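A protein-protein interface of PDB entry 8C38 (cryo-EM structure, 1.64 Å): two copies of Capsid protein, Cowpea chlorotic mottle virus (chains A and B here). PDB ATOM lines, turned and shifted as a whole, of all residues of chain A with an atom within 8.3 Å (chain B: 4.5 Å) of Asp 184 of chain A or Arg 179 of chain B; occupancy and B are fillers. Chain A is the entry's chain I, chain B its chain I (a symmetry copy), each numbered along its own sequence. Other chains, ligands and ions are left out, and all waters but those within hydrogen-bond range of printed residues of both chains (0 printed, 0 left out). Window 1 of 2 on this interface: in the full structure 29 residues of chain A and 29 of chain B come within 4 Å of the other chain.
O of Gly 49 of chain B is in hydrogen-bond range of N of Arg 179 of chain B (2.8 Å).
NE of Arg 179 of chain B lies within hydrogen-bond range of O of Tyr 50 of chain B (3.1 Å).
N of Ser 51 of chain B lies within hydrogen-bond range of O of His 177 of chain B (2.8 Å).
Printed residues of chain B within 4 Å of Asp 184 of chain A: Lys 45 (2.6 Å), Ala 46 (2.9 Å) and Arg 179 (2.5 Å).
No residue of chain A comes within 4 Å of Pro 180 of chain B.
Of the printed residues of chain B, Asp 183 of chain A touches Ser 51.
Printed residues of chain A within 4 Å of Ala 46 of chain B: Asp 184 (2.9 Å) and Ser 185 (3.9 Å).
Of the printed residues of chain B, Ser 185 of chain A touches Lys 45 (3.8 Å) and Ala 46 (3.9 Å).
Of the printed residues of chain A, Lys 45 of chain B touches Asp 184 and Ser 185.
Printed residues of chain A within 4 Å of Ser 51 of chain B: Asp 183 (3.8 Å).
Thr 181 of chain A touches none of the printed residues of chain B.
Phe 186 of chain A touches none of the printed residues of chain B.
The nearest printed residue of chain B that does not touch Asp 184 of chain A is Ser 51 of chain B (4.8 Å).
The nearest residue of chain A that does not touch Arg 179 of chain B is Pro 180 of chain A (5.1 Å).
Among the printed residues, merely in contact across the chains: Asp 183 of chain A with Ser 51 of chain B, Ser 185 of chain A with Lys 45 of chain B and Ser 185 of chain A with Ala 46 of chain B.
Positions printed for both chains: 179, 180 and 181.
NH2 of Arg 179 of chain B is in salt-bridge range of OD1 of Asp 184 of chain A.
The backbone NH (N) of Ala 46 of chain B lies within hydrogen-bond range of the backbone carbonyl oxygen (O) of Asp 184 of chain A (2.9 Å).
The backbone carbonyl oxygen (O) of Asp 184 of chain A is in hydrogen-bond range of the side-chain amino group (NZ) of Lys 45 of chain B (2.6 Å).
Of the 10 printed residues of chain A, 3 touch a printed residue of chain B.
Among the printed residues, 6 pairs touch across the chains.
Among the printed residues, Asp or Glu carboxylates within 4 Å of a Lys or Arg side-chain nitrogen of the other chain: Asp 184 of chain A with Arg 179 of chain B.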
ATOM      1  N   ARG A  82      15.166  11.919 -32.253  1.00  0.00           N
ATOM      2  CA  ARG A  82      13.736  12.204 -32.299  1.00  0.00           C
ATOM      3  C   ARG A  82      13.448  13.658 -31.941  1.00  0.00           C
ATOM      4  O   ARG A  82      12.637  14.318 -32.601  1.00  0.00           O
ATOM      5  CB  ARG A  82      12.983  11.273 -31.347  1.00  0.00           C
ATOM      6  CG  ARG A  82      12.776   9.845 -31.863  1.00  0.00           C
ATOM      7  CD  ARG A  82      11.610   9.753 -32.828  1.00  0.00           C
ATOM      8  NE  ARG A  82      10.339  10.127 -32.220  1.00  0.00           N
ATOM      9  CZ  ARG A  82       9.494   9.284 -31.641  1.00  0.00           C
ATOM     10  NH1 ARG A  82       9.752   7.988 -31.561  1.00  0.00           N
ATOM     11  NH2 ARG A  82       8.356   9.751 -31.136  1.00  0.00           N
ATOM     12  N   ARG A 179       5.630  18.862 -27.859  1.00  0.00           N
ATOM     13  CA  ARG A 179       6.030  18.035 -26.732  1.00  0.00           C
ATOM     14  C   ARG A 179       6.673  16.748 -27.243  1.00  0.00           C
ATOM     15  O   ARG A 179       6.084  16.065 -28.089  1.00  0.00           O
ATOM     16  CB  ARG A 179       4.828  17.704 -25.849  1.00  0.00           C
ATOM     17  CG  ARG A 179       4.274  18.893 -25.092  1.00  0.00           C
ATOM     18  CD  ARG A 179       3.161  18.478 -24.141  1.00  0.00           C
ATOM     19  NE  ARG A 179       2.746  19.581 -23.285  1.00  0.00           N
ATOM     20  CZ  ARG A 179       3.286  19.860 -22.106  1.00  0.00           C
ATOM     21  NH1 ARG A 179       4.268  19.128 -21.603  1.00  0.00           N
ATOM     22  NH2 ARG A 179       2.831  20.900 -21.414  1.00  0.00           N
ATOM     23  N   PRO A 180       7.870  16.392 -26.777  1.00  0.00           N
ATOM     24  CA  PRO A 180       8.440  15.096 -27.161  1.00  0.00           C
ATOM     25  C   PRO A 180       7.600  13.950 -26.616  1.00  0.00           C
ATOM     26  O   PRO A 180       7.072  14.017 -25.506  1.00  0.00           O
ATOM     27  CB  PRO A 180       9.842  15.120 -26.542  1.00  0.00           C
ATOM     28  CG  PRO A 180       9.804  16.167 -25.500  1.00  0.00           C
ATOM     29  CD  PRO A 180       8.784  17.170 -25.926  1.00  0.00           C
ATOM     30  N   THR A 181       7.487  12.886 -27.411  1.00  0.00           N
ATOM     31  CA  THR A 181       6.714  11.715 -27.022  1.00  0.00           C
ATOM     32  C   THR A 181       7.561  10.477 -26.771  1.00  0.00           C
ATOM     33  O   THR A 181       7.056   9.516 -26.183  1.00  0.00           O
ATOM     34  CB  THR A 181       5.676  11.375 -28.102  1.00  0.00           C
ATOM     35  OG1 THR A 181       6.311  11.360 -29.387  1.00  0.00           O
ATOM     36  CG2 THR A 181       4.542  12.390 -28.106  1.00  0.00           C
ATOM     37  N   PHE A 182       8.828  10.478 -27.185  1.00  0.00           N
ATOM     38  CA  PHE A 182       9.627   9.261 -27.097  1.00  0.00           C
ATOM     39  C   PHE A 182       9.821   8.812 -25.654  1.00  0.00           C
ATOM     40  O   PHE A 182      10.023   7.620 -25.400  1.00  0.00           O
ATOM     41  CB  PHE A 182      10.983   9.481 -27.766  1.00  0.00           C
ATOM     42  CG  PHE A 182      11.788   8.223 -27.941  1.00  0.00           C
ATOM     43  CD1 PHE A 182      11.183   7.041 -28.336  1.00  0.00           C
ATOM     44  CD2 PHE A 182      13.151   8.223 -27.712  1.00  0.00           C
ATOM     45  CE1 PHE A 182      11.923   5.887 -28.498  1.00  0.00           C
ATOM     46  CE2 PHE A 182      13.894   7.069 -27.877  1.00  0.00           C
ATOM     47  CZ  PHE A 182      13.277   5.903 -28.268  1.00  0.00           C
ATOM     48  N   ASP A 183       9.751   9.741 -24.701  1.00  0.00           N
ATOM     49  CA  ASP A 183       9.972   9.447 -23.292  1.00  0.00           C
ATOM     50  C   ASP A 183       8.679   9.146 -22.539  1.00  0.00           C
ATOM     51  O   ASP A 183       8.666   9.194 -21.304  1.00  0.00           O
ATOM     52  CB  ASP A 183      10.704  10.615 -22.625  1.00  0.00           C
ATOM     53  CG  ASP A 183      12.175  10.679 -23.002  1.00  0.00           C
ATOM     54  OD1 ASP A 183      12.717   9.669 -23.499  1.00  0.00           O
ATOM     55  OD2 ASP A 183      12.788  11.749 -22.807  1.00  0.00           O
ATOM     56  N   ASP A 184       7.594   8.849 -23.250  1.00  0.00           N
ATOM     57  CA  ASP A 184       6.354   8.436 -22.612  1.00  0.00           C
ATOM     58  C   ASP A 184       6.335   6.950 -22.271  1.00  0.00           C
ATOM     59  O   ASP A 184       5.298   6.443 -21.833  1.00  0.00           O
ATOM     60  CB  ASP A 184       5.162   8.780 -23.511  1.00  0.00           C
ATOM     61  CG  ASP A 184       5.017  10.278 -23.732  1.00  0.00           C
ATOM     62  OD1 ASP A 184       5.685  11.050 -23.016  1.00  0.00           O
ATOM     63  OD2 ASP A 184       4.238  10.681 -24.621  1.00  0.00           O
ATOM     64  N   SER A 185       7.450   6.246 -22.447  1.00  0.00           N
ATOM     65  CA  SER A 185       7.518   4.830 -22.123  1.00  0.00           C
ATOM     66  C   SER A 185       8.963   4.452 -21.832  1.00  0.00           C
ATOM     67  O   SER A 185       9.898   5.159 -22.213  1.00  0.00           O
ATOM     68  CB  SER A 185       6.964   3.971 -23.264  1.00  0.00           C
ATOM     69  OG  SER A 185       7.762   4.105 -24.425  1.00  0.00           O
ATOM     70  N   PHE A 186       9.131   3.322 -21.151  1.00  0.00           N
ATOM     71  CA  PHE A 186      10.453   2.765 -20.916  1.00  0.00           C
ATOM     72  C   PHE A 186      11.004   2.151 -22.199  1.00  0.00           C
ATOM     73  O   PHE A 186      10.262   1.802 -23.118  1.00  0.00           O
ATOM     74  CB  PHE A 186      10.398   1.693 -19.827  1.00  0.00           C
ATOM     75  CG  PHE A 186      10.135   2.238 -18.453  1.00  0.00           C
ATOM     76  CD1 PHE A 186      11.181   2.638 -17.643  1.00  0.00           C
ATOM     77  CD2 PHE A 186       8.843   2.351 -17.977  1.00  0.00           C
ATOM     78  CE1 PHE A 186      10.944   3.137 -16.374  1.00  0.00           C
ATOM     79  CE2 PHE A 186       8.601   2.848 -16.712  1.00  0.00           C
ATOM     80  CZ  PHE A 186       9.654   3.243 -15.914  1.00  0.00           C
ATOM     81  N   THR A 187      12.322   2.008 -22.243  1.00  0.00           N
ATOM     82  CA  THR A 187      12.944   1.223 -23.297  1.00  0.00           C
ATOM     83  C   THR A 187      12.500  -0.227 -23.147  1.00  0.00           C
ATOM     84  O   THR A 187      12.512  -0.755 -22.029  1.00  0.00           O
ATOM     85  CB  THR A 187      14.466   1.310 -23.209  1.00  0.00           C
ATOM     86  OG1 THR A 187      14.873   2.681 -23.240  1.00  0.00           O
ATOM     87  CG2 THR A 187      15.121   0.546 -24.356  1.00  0.00           C
ATOM     88  N   LYS B  45       4.494   1.492 -20.969  1.00  0.00           N
ATOM     89  CA  LYS B  45       4.024   2.864 -21.065  1.00  0.00           C
ATOM     90  C   LYS B  45       4.024   3.522 -19.692  1.00  0.00           C
ATOM     91  O   LYS B  45       3.641   2.908 -18.695  1.00  0.00           O
ATOM     92  CB  LYS B  45       2.616   2.896 -21.661  1.00  0.00           C
ATOM     93  CG  LYS B  45       2.041   4.288 -21.875  1.00  0.00           C
ATOM     94  CD  LYS B  45       2.852   5.111 -22.862  1.00  0.00           C
ATOM     95  CE  LYS B  45       2.267   6.506 -23.034  1.00  0.00           C
ATOM     96  NZ  LYS B  45       2.881   7.488 -22.098  1.00  0.00           N
ATOM     97  N   ALA B  46       4.441   4.783 -19.650  1.00  0.00           N
ATOM     98  CA  ALA B  46       4.400   5.532 -18.402  1.00  0.00           C
ATOM     99  C   ALA B  46       2.958   5.693 -17.933  1.00  0.00           C
ATOM    100  O   ALA B  46       2.020   5.689 -18.731  1.00  0.00           O
ATOM    101  CB  ALA B  46       5.048   6.904 -18.581  1.00  0.00           C
ATOM    102  N   GLY B  49      -0.021  11.027 -16.593  1.00  0.00           N
ATOM    103  CA  GLY B  49       0.561  12.103 -15.825  1.00  0.00           C
ATOM    104  C   GLY B  49       2.024  11.924 -15.491  1.00  0.00           C
ATOM    105  O   GLY B  49       2.612  12.817 -14.869  1.00  0.00           O
ATOM    106  N   TYR B  50       2.627  10.807 -15.881  1.00  0.00           N
ATOM    107  CA  TYR B  50       4.040  10.545 -15.669  1.00  0.00           C
ATOM    108  C   TYR B  50       4.779  10.542 -17.000  1.00  0.00           C
ATOM    109  O   TYR B  50       4.193  10.344 -18.066  1.00  0.00           O
ATOM    110  CB  TYR B  50       4.253   9.199 -14.971  1.00  0.00           C
ATOM    111  CG  TYR B  50       3.889   9.197 -13.509  1.00  0.00           C
ATOM    112  CD1 TYR B  50       2.569   9.304 -13.100  1.00  0.00           C
ATOM    113  CD2 TYR B  50       4.868   9.083 -12.538  1.00  0.00           C
ATOM    114  CE1 TYR B  50       2.238   9.301 -11.760  1.00  0.00           C
ATOM    115  CE2 TYR B  50       4.550   9.079 -11.199  1.00  0.00           C
ATOM    116  CZ  TYR B  50       3.234   9.184 -10.813  1.00  0.00           C
ATOM    117  OH  TYR B  50       2.915   9.179  -9.477  1.00  0.00           O
ATOM    118  N   SER B  51       6.086  10.772 -16.918  1.00  0.00           N
ATOM    119  CA  SER B  51       6.998  10.609 -18.036  1.00  0.00           C
ATOM    120  C   SER B  51       8.218   9.842 -17.546  1.00  0.00           C
ATOM    121  O   SER B  51       8.451   9.708 -16.344  1.00  0.00           O
ATOM    122  CB  SER B  51       7.414  11.960 -18.630  1.00  0.00           C
ATOM    123  OG  SER B  51       8.068  12.751 -17.658  1.00  0.00           O
ATOM    124  N   LEU B  86       9.362  16.190  -7.901  1.00  0.00           N
ATOM    125  CA  LEU B  86       8.457  15.312  -8.626  1.00  0.00           C
ATOM    126  C   LEU B  86       8.550  13.891  -8.090  1.00  0.00           C
ATOM    127  O   LEU B  86       9.641  13.366  -7.864  1.00  0.00           O
ATOM    128  CB  LEU B  86       8.787  15.331 -10.115  1.00  0.00           C
ATOM    129  CG  LEU B  86       8.617  16.702 -10.774  1.00  0.00           C
ATOM    130  CD1 LEU B  86       9.323  16.742 -12.121  1.00  0.00           C
ATOM    131  CD2 LEU B  86       7.148  17.035 -10.917  1.00  0.00           C
ATOM    132  N   HIS B 177       8.420   9.441 -13.516  1.00  0.00           N
ATOM    133  CA  HIS B 177       8.127  10.463 -12.522  1.00  0.00           C
ATOM    134  C   HIS B 177       7.014  11.363 -13.036  1.00  0.00           C
ATOM    135  O   HIS B 177       6.703  11.383 -14.227  1.00  0.00           O
ATOM    136  CB  HIS B 177       9.374  11.283 -12.188  1.00  0.00           C
ATOM    137  CG  HIS B 177       9.933  12.023 -13.359  1.00  0.00           C
ATOM    138  ND1 HIS B 177       9.350  13.167 -13.863  1.00  0.00           N
ATOM    139  CD2 HIS B 177      11.017  11.781 -14.132  1.00  0.00           C
ATOM    140  CE1 HIS B 177      10.054  13.597 -14.895  1.00  0.00           C
ATOM    141  NE2 HIS B 177      11.071  12.775 -15.079  1.00  0.00           N
ATOM    142  N   VAL B 178       6.407  12.100 -12.105  1.00  0.00           N
ATOM    143  CA  VAL B 178       5.323  12.999 -12.473  1.00  0.00           C
ATOM    144  C   VAL B 178       5.818  13.980 -13.522  1.00  0.00           C
ATOM    145  O   VAL B 178       6.946  14.480 -13.450  1.00  0.00           O
ATOM    146  CB  VAL B 178       4.792  13.724 -11.226  1.00  0.00           C
ATOM    147  CG1 VAL B 178       3.800  14.809 -11.619  1.00  0.00           C
ATOM    148  CG2 VAL B 178       4.156  12.722 -10.283  1.00  0.00           C
ATOM    149  N   ARG B 179       4.980  14.243 -14.515  1.00  0.00           N
ATOM    150  CA  ARG B 179       5.361  15.169 -15.570  1.00  0.00           C
ATOM    151  C   ARG B 179       5.561  16.563 -14.981  1.00  0.00           C
ATOM    152  O   ARG B 179       4.678  17.059 -14.272  1.00  0.00           O
ATOM    153  CB  ARG B 179       4.294  15.211 -16.663  1.00  0.00           C
ATOM    154  CG  ARG B 179       4.198  13.940 -17.481  1.00  0.00           C
ATOM    155  CD  ARG B 179       3.208  14.089 -18.626  1.00  0.00           C
ATOM    156  NE  ARG B 179       3.240  12.937 -19.518  1.00  0.00           N
ATOM    157  CZ  ARG B 179       4.036  12.827 -20.573  1.00  0.00           C
ATOM    158  NH1 ARG B 179       4.881  13.791 -20.907  1.00  0.00           N
ATOM    159  NH2 ARG B 179       3.986  11.723 -21.312  1.00  0.00           N
ATOM    160  N   PRO B 180       6.696  17.215 -15.231  1.00  0.00           N
ATOM    161  CA  PRO B 180       6.848  18.603 -14.781  1.00  0.00           C
ATOM    162  C   PRO B 180       5.864  19.516 -15.494  1.00  0.00           C
ATOM    163  O   PRO B 180       5.578  19.346 -16.680  1.00  0.00           O
ATOM    164  CB  PRO B 180       8.301  18.941 -15.136  1.00  0.00           C
ATOM    165  CG  PRO B 180       8.712  17.940 -16.142  1.00  0.00           C
ATOM    166  CD  PRO B 180       7.913  16.707 -15.885  1.00  0.00           C
ATOM    167  N   THR B 181       5.349  20.501 -14.758  1.00  0.00           N
ATOM    168  CA  THR B 181       4.393  21.453 -15.306  1.00  0.00           C
ATOM    169  C   THR B 181       4.938  22.867 -15.429  1.00  0.00           C
ATOM    170  O   THR B 181       4.325  23.686 -16.120  1.00  0.00           O
ATOM    171  CB  THR B 181       3.126  21.500 -14.440  1.00  0.00           C
ATOM    172  OG1 THR B 181       3.494  21.642 -13.062  1.00  0.00           O
ATOM    173  CG2 THR B 181       2.296  20.236 -14.617  1.00  0.00           C
